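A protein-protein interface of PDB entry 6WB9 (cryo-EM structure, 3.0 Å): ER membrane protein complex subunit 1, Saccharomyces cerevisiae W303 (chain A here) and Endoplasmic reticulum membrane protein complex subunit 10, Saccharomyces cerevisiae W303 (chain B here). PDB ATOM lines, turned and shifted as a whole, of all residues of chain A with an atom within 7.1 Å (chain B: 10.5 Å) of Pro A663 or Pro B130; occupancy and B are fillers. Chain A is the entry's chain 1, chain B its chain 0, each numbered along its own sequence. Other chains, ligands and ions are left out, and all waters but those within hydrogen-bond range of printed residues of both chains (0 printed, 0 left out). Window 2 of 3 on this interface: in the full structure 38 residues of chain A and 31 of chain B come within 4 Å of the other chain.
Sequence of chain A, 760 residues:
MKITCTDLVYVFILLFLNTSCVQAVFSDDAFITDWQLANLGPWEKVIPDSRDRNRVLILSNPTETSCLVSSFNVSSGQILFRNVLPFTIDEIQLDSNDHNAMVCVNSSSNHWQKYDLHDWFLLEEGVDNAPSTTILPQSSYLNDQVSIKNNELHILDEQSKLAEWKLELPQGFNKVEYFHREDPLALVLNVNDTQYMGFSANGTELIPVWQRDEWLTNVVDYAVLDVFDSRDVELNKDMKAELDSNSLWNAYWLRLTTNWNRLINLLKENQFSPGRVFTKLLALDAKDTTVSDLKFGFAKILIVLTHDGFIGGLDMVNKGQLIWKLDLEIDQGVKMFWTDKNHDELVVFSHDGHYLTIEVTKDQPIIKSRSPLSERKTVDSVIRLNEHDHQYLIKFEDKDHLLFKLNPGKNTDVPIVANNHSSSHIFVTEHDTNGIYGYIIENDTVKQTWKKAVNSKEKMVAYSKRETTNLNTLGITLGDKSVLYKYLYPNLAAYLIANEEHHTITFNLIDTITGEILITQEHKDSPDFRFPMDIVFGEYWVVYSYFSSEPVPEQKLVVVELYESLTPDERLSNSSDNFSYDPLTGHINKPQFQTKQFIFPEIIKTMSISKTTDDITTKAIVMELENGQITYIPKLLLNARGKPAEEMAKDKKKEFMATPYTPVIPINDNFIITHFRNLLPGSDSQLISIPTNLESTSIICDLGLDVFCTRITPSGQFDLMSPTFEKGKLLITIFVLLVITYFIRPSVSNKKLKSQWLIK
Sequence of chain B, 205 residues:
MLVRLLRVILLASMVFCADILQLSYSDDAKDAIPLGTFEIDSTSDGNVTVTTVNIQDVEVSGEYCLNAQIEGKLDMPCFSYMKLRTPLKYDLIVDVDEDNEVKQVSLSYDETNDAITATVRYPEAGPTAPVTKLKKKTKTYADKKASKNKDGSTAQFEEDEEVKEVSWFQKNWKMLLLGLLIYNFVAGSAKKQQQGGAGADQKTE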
ATOM      1  N   PRO A 551     -35.714  -2.074  24.249  1.00  0.00           N
ATOM      2  CA  PRO A 551     -35.944  -1.046  23.221  1.00  0.00           C
ATOM      3  C   PRO A 551     -36.038  -1.669  21.841  1.00  0.00           C
ATOM      4  O   PRO A 551     -37.025  -1.496  21.120  1.00  0.00           O
ATOM      5  CB  PRO A 551     -34.718  -0.129  23.336  1.00  0.00           C
ATOM      6  CG  PRO A 551     -34.028  -0.532  24.568  1.00  0.00           C
ATOM      7  CD  PRO A 551     -34.336  -1.962  24.770  1.00  0.00           C
ATOM      8  N   LYS A 596     -24.837   6.818  28.966  1.00  0.00           N
ATOM      9  CA  LYS A 596     -25.616   6.694  27.744  1.00  0.00           C
ATOM     10  C   LYS A 596     -25.673   5.233  27.338  1.00  0.00           C
ATOM     11  O   LYS A 596     -24.780   4.452  27.660  1.00  0.00           O
ATOM     12  CB  LYS A 596     -25.035   7.516  26.590  1.00  0.00           C
ATOM     13  CG  LYS A 596     -25.288   9.003  26.685  1.00  0.00           C
ATOM     14  CD  LYS A 596     -26.748   9.334  26.867  1.00  0.00           C
ATOM     15  CE  LYS A 596     -26.921  10.777  27.280  1.00  0.00           C
ATOM     16  NZ  LYS A 596     -28.334  11.073  27.617  1.00  0.00           N
ATOM     17  N   GLN A 597     -26.739   4.865  26.641  1.00  0.00           N
ATOM     18  CA  GLN A 597     -26.857   3.547  26.041  1.00  0.00           C
ATOM     19  C   GLN A 597     -26.932   3.703  24.532  1.00  0.00           C
ATOM     20  O   GLN A 597     -27.596   4.609  24.024  1.00  0.00           O
ATOM     21  CB  GLN A 597     -28.084   2.794  26.551  1.00  0.00           C
ATOM     22  CG  GLN A 597     -28.081   1.323  26.206  1.00  0.00           C
ATOM     23  CD  GLN A 597     -29.416   0.663  26.430  1.00  0.00           C
ATOM     24  OE1 GLN A 597     -30.402   1.004  25.786  1.00  0.00           O
ATOM     25  NE2 GLN A 597     -29.455  -0.295  27.341  1.00  0.00           N
ATOM     26  N   PHE A 598     -26.234   2.825  23.824  1.00  0.00           N
ATOM     27  CA  PHE A 598     -26.158   2.825  22.376  1.00  0.00           C
ATOM     28  C   PHE A 598     -26.582   1.459  21.874  1.00  0.00           C
ATOM     29  O   PHE A 598     -26.296   0.443  22.508  1.00  0.00           O
ATOM     30  CB  PHE A 598     -24.737   3.125  21.889  1.00  0.00           C
ATOM     31  CG  PHE A 598     -24.183   4.439  22.362  1.00  0.00           C
ATOM     32  CD1 PHE A 598     -24.325   5.576  21.591  1.00  0.00           C
ATOM     33  CD2 PHE A 598     -23.499   4.532  23.560  1.00  0.00           C
ATOM     34  CE1 PHE A 598     -23.815   6.780  22.012  1.00  0.00           C
ATOM     35  CE2 PHE A 598     -22.991   5.734  23.984  1.00  0.00           C
ATOM     36  CZ  PHE A 598     -23.148   6.856  23.208  1.00  0.00           C
ATOM     37  N   ILE A 599     -27.276   1.429  20.750  1.00  0.00           N
ATOM     38  CA  ILE A 599     -27.521   0.162  20.085  1.00  0.00           C
ATOM     39  C   ILE A 599     -26.317  -0.168  19.205  1.00  0.00           C
ATOM     40  O   ILE A 599     -25.449   0.667  18.961  1.00  0.00           O
ATOM     41  CB  ILE A 599     -28.836   0.199  19.280  1.00  0.00           C
ATOM     42  CG1 ILE A 599     -29.874   1.084  19.973  1.00  0.00           C
ATOM     43  CG2 ILE A 599     -29.463  -1.175  19.178  1.00  0.00           C
ATOM     44  CD1 ILE A 599     -30.461   0.525  21.263  1.00  0.00           C
ATOM     45  N   PHE A 600     -26.225  -1.418  18.796  1.00  0.00           N
ATOM     46  CA  PHE A 600     -25.174  -1.915  17.931  1.00  0.00           C
ATOM     47  C   PHE A 600     -25.735  -3.132  17.208  1.00  0.00           C
ATOM     48  O   PHE A 600     -26.386  -3.984  17.836  1.00  0.00           O
ATOM     49  CB  PHE A 600     -23.918  -2.253  18.736  1.00  0.00           C
ATOM     50  CG  PHE A 600     -22.673  -2.336  17.907  1.00  0.00           C
ATOM     51  CD1 PHE A 600     -22.090  -1.191  17.400  1.00  0.00           C
ATOM     52  CD2 PHE A 600     -22.086  -3.558  17.635  1.00  0.00           C
ATOM     53  CE1 PHE A 600     -20.948  -1.263  16.635  1.00  0.00           C
ATOM     54  CE2 PHE A 600     -20.942  -3.635  16.869  1.00  0.00           C
ATOM     55  CZ  PHE A 600     -20.374  -2.486  16.370  1.00  0.00           C
ATOM     56  N   PRO A 644     -28.570  15.167  21.729  1.00  0.00           N
ATOM     57  CA  PRO A 644     -28.856  14.837  20.326  1.00  0.00           C
ATOM     58  C   PRO A 644     -28.629  16.027  19.404  1.00  0.00           C
ATOM     59  O   PRO A 644     -28.465  17.169  19.839  1.00  0.00           O
ATOM     60  CB  PRO A 644     -30.328  14.421  20.351  1.00  0.00           C
ATOM     61  CG  PRO A 644     -30.871  15.018  21.597  1.00  0.00           C
ATOM     62  CD  PRO A 644     -29.755  14.982  22.581  1.00  0.00           C
ATOM     63  N   PRO A 660     -22.423  14.401  18.940  1.00  0.00           N
ATOM     64  CA  PRO A 660     -23.744  14.315  19.563  1.00  0.00           C
ATOM     65  C   PRO A 660     -24.026  12.901  20.054  1.00  0.00           C
ATOM     66  O   PRO A 660     -23.240  11.975  19.872  1.00  0.00           O
ATOM     67  CB  PRO A 660     -24.687  14.713  18.428  1.00  0.00           C
ATOM     68  CG  PRO A 660     -23.967  14.317  17.202  1.00  0.00           C
ATOM     69  CD  PRO A 660     -22.521  14.579  17.481  1.00  0.00           C
ATOM     70  N   TYR A 661     -25.180  12.748  20.691  1.00  0.00           N
ATOM     71  CA  TYR A 661     -25.644  11.440  21.137  1.00  0.00           C
ATOM     72  C   TYR A 661     -26.342  10.771  19.963  1.00  0.00           C
ATOM     73  O   TYR A 661     -27.488  11.091  19.641  1.00  0.00           O
ATOM     74  CB  TYR A 661     -26.571  11.581  22.335  1.00  0.00           C
ATOM     75  CG  TYR A 661     -27.112  10.285  22.877  1.00  0.00           C
ATOM     76  CD1 TYR A 661     -26.308   9.161  22.984  1.00  0.00           C
ATOM     77  CD2 TYR A 661     -28.427  10.193  23.306  1.00  0.00           C
ATOM     78  CE1 TYR A 661     -26.805   7.977  23.482  1.00  0.00           C
ATOM     79  CE2 TYR A 661     -28.931   9.015  23.811  1.00  0.00           C
ATOM     80  CZ  TYR A 661     -28.114   7.914  23.903  1.00  0.00           C
ATOM     81  OH  TYR A 661     -28.613   6.736  24.401  1.00  0.00           O
ATOM     82  N   THR A 662     -25.633   9.860  19.300  1.00  0.00           N
ATOM     83  CA  THR A 662     -26.209   9.021  18.261  1.00  0.00           C
ATOM     84  C   THR A 662     -26.413   7.634  18.845  1.00  0.00           C
ATOM     85  O   THR A 662     -25.474   6.827  18.846  1.00  0.00           O
ATOM     86  CB  THR A 662     -25.295   8.960  17.036  1.00  0.00           C
ATOM     87  OG1 THR A 662     -24.051   8.351  17.400  1.00  0.00           O
ATOM     88  CG2 THR A 662     -25.032  10.355  16.493  1.00  0.00           C
ATOM     89  N   PRO A 663     -27.603   7.303  19.361  1.00  0.00           N
ATOM     90  CA  PRO A 663     -27.825   6.011  20.016  1.00  0.00           C
ATOM     91  C   PRO A 663     -28.204   4.895  19.053  1.00  0.00           C
ATOM     92  O   PRO A 663     -29.139   4.136  19.295  1.00  0.00           O
ATOM     93  CB  PRO A 663     -28.985   6.317  20.964  1.00  0.00           C
ATOM     94  CG  PRO A 663     -29.794   7.295  20.193  1.00  0.00           C
ATOM     95  CD  PRO A 663     -28.823   8.126  19.383  1.00  0.00           C
ATOM     96  N   VAL A 664     -27.506   4.813  17.925  1.00  0.00           N
ATOM     97  CA  VAL A 664     -27.738   3.781  16.926  1.00  0.00           C
ATOM     98  C   VAL A 664     -26.450   3.047  16.577  1.00  0.00           C
ATOM     99  O   VAL A 664     -26.409   1.814  16.583  1.00  0.00           O
ATOM    100  CB  VAL A 664     -28.410   4.361  15.661  1.00  0.00           C
ATOM    101  CG1 VAL A 664     -28.280   3.426  14.476  1.00  0.00           C
ATOM    102  CG2 VAL A 664     -29.880   4.622  15.941  1.00  0.00           C
ATOM    103  N   ILE A 665     -25.375   3.797  16.325  1.00  0.00           N
ATOM    104  CA  ILE A 665     -24.036   3.314  15.966  1.00  0.00           C
ATOM    105  C   ILE A 665     -24.096   2.350  14.784  1.00  0.00           C
ATOM    106  O   ILE A 665     -24.086   1.127  14.987  1.00  0.00           O
ATOM    107  CB  ILE A 665     -23.313   2.670  17.163  1.00  0.00           C
ATOM    108  CG1 ILE A 665     -23.466   3.523  18.418  1.00  0.00           C
ATOM    109  CG2 ILE A 665     -21.835   2.522  16.859  1.00  0.00           C
ATOM    110  CD1 ILE A 665     -22.767   4.862  18.353  1.00  0.00           C
ATOM    111  N   PRO A 666     -24.250   2.838  13.555  1.00  0.00           N
ATOM    112  CA  PRO A 666     -24.189   1.939  12.402  1.00  0.00           C
ATOM    113  C   PRO A 666     -22.788   1.378  12.239  1.00  0.00           C
ATOM    114  O   PRO A 666     -21.792   2.031  12.557  1.00  0.00           O
ATOM    115  CB  PRO A 666     -24.571   2.843  11.227  1.00  0.00           C
ATOM    116  CG  PRO A 666     -24.132   4.195  11.660  1.00  0.00           C
ATOM    117  CD  PRO A 666     -24.349   4.250  13.145  1.00  0.00           C
ATOM    118  N   GLY B 126     -30.454   2.249  34.657  1.00  0.00           N
ATOM    119  CA  GLY B 126     -29.520   2.386  33.571  1.00  0.00           C
ATOM    120  C   GLY B 126     -30.167   3.094  32.406  1.00  0.00           C
ATOM    121  O   GLY B 126     -31.395   3.141  32.287  1.00  0.00           O
ATOM    122  N   PRO B 127     -29.354   3.675  31.530  1.00  0.00           N
ATOM    123  CA  PRO B 127     -29.908   4.447  30.421  1.00  0.00           C
ATOM    124  C   PRO B 127     -30.546   3.550  29.379  1.00  0.00           C
ATOM    125  O   PRO B 127     -30.176   2.387  29.208  1.00  0.00           O
ATOM    126  CB  PRO B 127     -28.687   5.171  29.855  1.00  0.00           C
ATOM    127  CG  PRO B 127     -27.577   4.272  30.168  1.00  0.00           C
ATOM    128  CD  PRO B 127     -27.883   3.671  31.501  1.00  0.00           C
ATOM    129  N   THR B 128     -31.538   4.105  28.698  1.00  0.00           N
ATOM    130  CA  THR B 128     -32.223   3.435  27.610  1.00  0.00           C
ATOM    131  C   THR B 128     -32.007   4.257  26.351  1.00  0.00           C
ATOM    132  O   THR B 128     -31.981   5.490  26.408  1.00  0.00           O
ATOM    133  CB  THR B 128     -33.713   3.281  27.910  1.00  0.00           C
ATOM    134  OG1 THR B 128     -33.887   2.962  29.295  1.00  0.00           O
ATOM    135  CG2 THR B 128     -34.305   2.166  27.087  1.00  0.00           C
ATOM    136  N   ALA B 129     -31.834   3.577  25.224  1.00  0.00           N
ATOM    137  CA  ALA B 129     -31.539   4.434  24.086  1.00  0.00           C
ATOM    138  C   ALA B 129     -32.828   4.878  23.399  1.00  0.00           C
ATOM    139  O   ALA B 129     -33.764   4.087  23.264  1.00  0.00           O
ATOM    140  CB  ALA B 129     -30.652   3.715  23.083  1.00  0.00           C
ATOM    141  N   PRO B 130     -32.896   6.136  22.979  1.00  0.00           N
ATOM    142  CA  PRO B 130     -34.045   6.586  22.188  1.00  0.00           C
ATOM    143  C   PRO B 130     -33.986   6.097  20.748  1.00  0.00           C
ATOM    144  O   PRO B 130     -33.517   6.812  19.857  1.00  0.00           O
ATOM    145  CB  PRO B 130     -33.951   8.112  22.272  1.00  0.00           C
ATOM    146  CG  PRO B 130     -32.531   8.391  22.572  1.00  0.00           C
ATOM    147  CD  PRO B 130     -32.052   7.260  23.414  1.00  0.00           C
ATOM    148  N   VAL B 131     -34.453   4.869  20.513  1.00  0.00           N
ATOM    149  CA  VAL B 131     -34.546   4.365  19.149  1.00  0.00           C
ATOM    150  C   VAL B 131     -35.692   5.055  18.415  1.00  0.00           C
ATOM    151  O   VAL B 131     -36.545   5.721  19.012  1.00  0.00           O
ATOM    152  CB  VAL B 131     -34.722   2.840  19.141  1.00  0.00           C
ATOM    153  CG1 VAL B 131     -33.564   2.179  19.850  1.00  0.00           C
ATOM    154  CG2 VAL B 131     -36.038   2.458  19.791  1.00  0.00           C
ATOM    155  N   THR B 132     -35.698   4.897  17.093  1.00  0.00           N
ATOM    156  CA  THR B 132     -36.735   5.495  16.264  1.00  0.00           C
ATOM    157  C   THR B 132     -38.074   4.813  16.513  1.00  0.00           C
ATOM    158  O   THR B 132     -38.163   3.585  16.568  1.00  0.00           O
ATOM    159  CB  THR B 132     -36.362   5.387  14.787  1.00  0.00           C
ATOM    160  OG1 THR B 132     -34.992   5.768  14.613  1.00  0.00           O
ATOM    161  CG2 THR B 132     -37.231   6.294  13.945  1.00  0.00           C
ATOM    162  N   LYS B 133     -39.116   5.617  16.679  1.00  0.00           N
ATOM    163  CA  LYS B 133     -40.447   5.106  16.956  1.00  0.00           C
ATOM    164  C   LYS B 133     -41.250   4.981  15.668  1.00  0.00           C
ATOM    165  O   LYS B 133     -40.855   5.457  14.602  1.00  0.00           O
ATOM    166  CB  LYS B 133     -41.181   6.007  17.954  1.00  0.00           C
ATOM    167  CG  LYS B 133     -40.933   5.667  19.418  1.00  0.00           C
ATOM    168  CD  LYS B 133     -39.660   6.305  19.933  1.00  0.00           C
ATOM    169  CE  LYS B 133     -39.297   5.787  21.311  1.00  0.00           C
ATOM    170  NZ  LYS B 133     -37.991   6.332  21.775  1.00  0.00           N
ATOM    171  N   LEU B 134     -42.399   4.323  15.782  1.00  0.00           N
ATOM    172  CA  LEU B 134     -43.336   4.168  14.679  1.00  0.00           C
ATOM    173  C   LEU B 134     -44.336   5.314  14.757  1.00  0.00           C
ATOM    174  O   LEU B 134     -45.225   5.317  15.614  1.00  0.00           O
ATOM    175  CB  LEU B 134     -44.033   2.810  14.743  1.00  0.00           C
ATOM    176  CG  LEU B 134     -43.538   1.723  13.787  1.00  0.00           C
ATOM    177  CD1 LEU B 134     -42.039   1.571  13.853  1.00  0.00           C
ATOM    178  CD2 LEU B 134     -44.211   0.404  14.102  1.00  0.00           C
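Hydrophobic or aromatic side chains of chain A within 4 Å of the printed part of chain B: Pro A551, Ile A599, Tyr A661 and Pro A663. Of the 9 printed residues of chain B, 5 touch a printed residue of chain A. Hydrophobic or aromatic side chains of chain B within 4 Å of the printed part of chain A: Pro B127, Ala B129, Pro B130 and Val B131. Along chain B the printed residues that touch a printed residue of chain A span positions 127 to 131.
The side-chain amino group (NZ) of Lys B133 sits at hydrogen-bond distance from the backbone carbonyl oxygen (O) of Val B131 (3.2 Å). The side-chain hydroxyl of Tyr A661 sits at hydrogen-bond distance from the backbone NH of Gln A597, at 3.5 Å.
Among the printed residues, merely in contact across the chains: Pro A551 with Thr B128 (3.7 Å), Lys A596 with Pro B127 (3.5 Å), Gln A597 with Thr B128 (3.5 Å), Ile A599 with Ala B129 (3.7 Å), Ile A599 with Val B131 (3.8 Å), Tyr A661 with Ala B129 (3.7 Å), Tyr A661 with Pro B130 (3.6 Å), Pro A663 with Ala B129 (3.7 Å) and Pro A663 with Pro B130 (3.8 Å).
The side-chain amide nitrogen (NE2) of Gln A597 is in hydrogen-bond range of the backbone carbonyl oxygen (O) of Pro B127, 3.3 Å away. The side-chain amide oxygen of Gln A597 lies within hydrogen-bond range of the backbone NH of Ala B129, 3.0 Å away.
Pro A663 touches just these residues of chain B: Ala B129 and Pro B130. No residue of chain B comes within 4 Å of Phe A598. Of the printed residues of chain B, Tyr A661 touches Ala B129 (3.7 Å) and Pro B130 (3.6 Å). Thr A662 touches none of the printed residues of chain B. No residue of chain B comes within 4 Å of Val A664. Of the printed residues of chain B, Lys A596 touches Pro B127. Of the printed residues of chain B, Pro A551 touches Thr B128 (3.7 Å). Of the printed residues of chain A, Pro B127 touches Lys A596 (3.5 Å) and Gln A597 (3.3 Å). Ile A665 touches none of the printed residues of chain B. Phe A600 touches none of the printed residues of chain B. The nearest residue of chain A that does not touch Pro B130 is Gln A597 (5.2 Å). The nearest printed residue of chain A that does not touch Val B131 is Pro A551 (4.3 Å).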
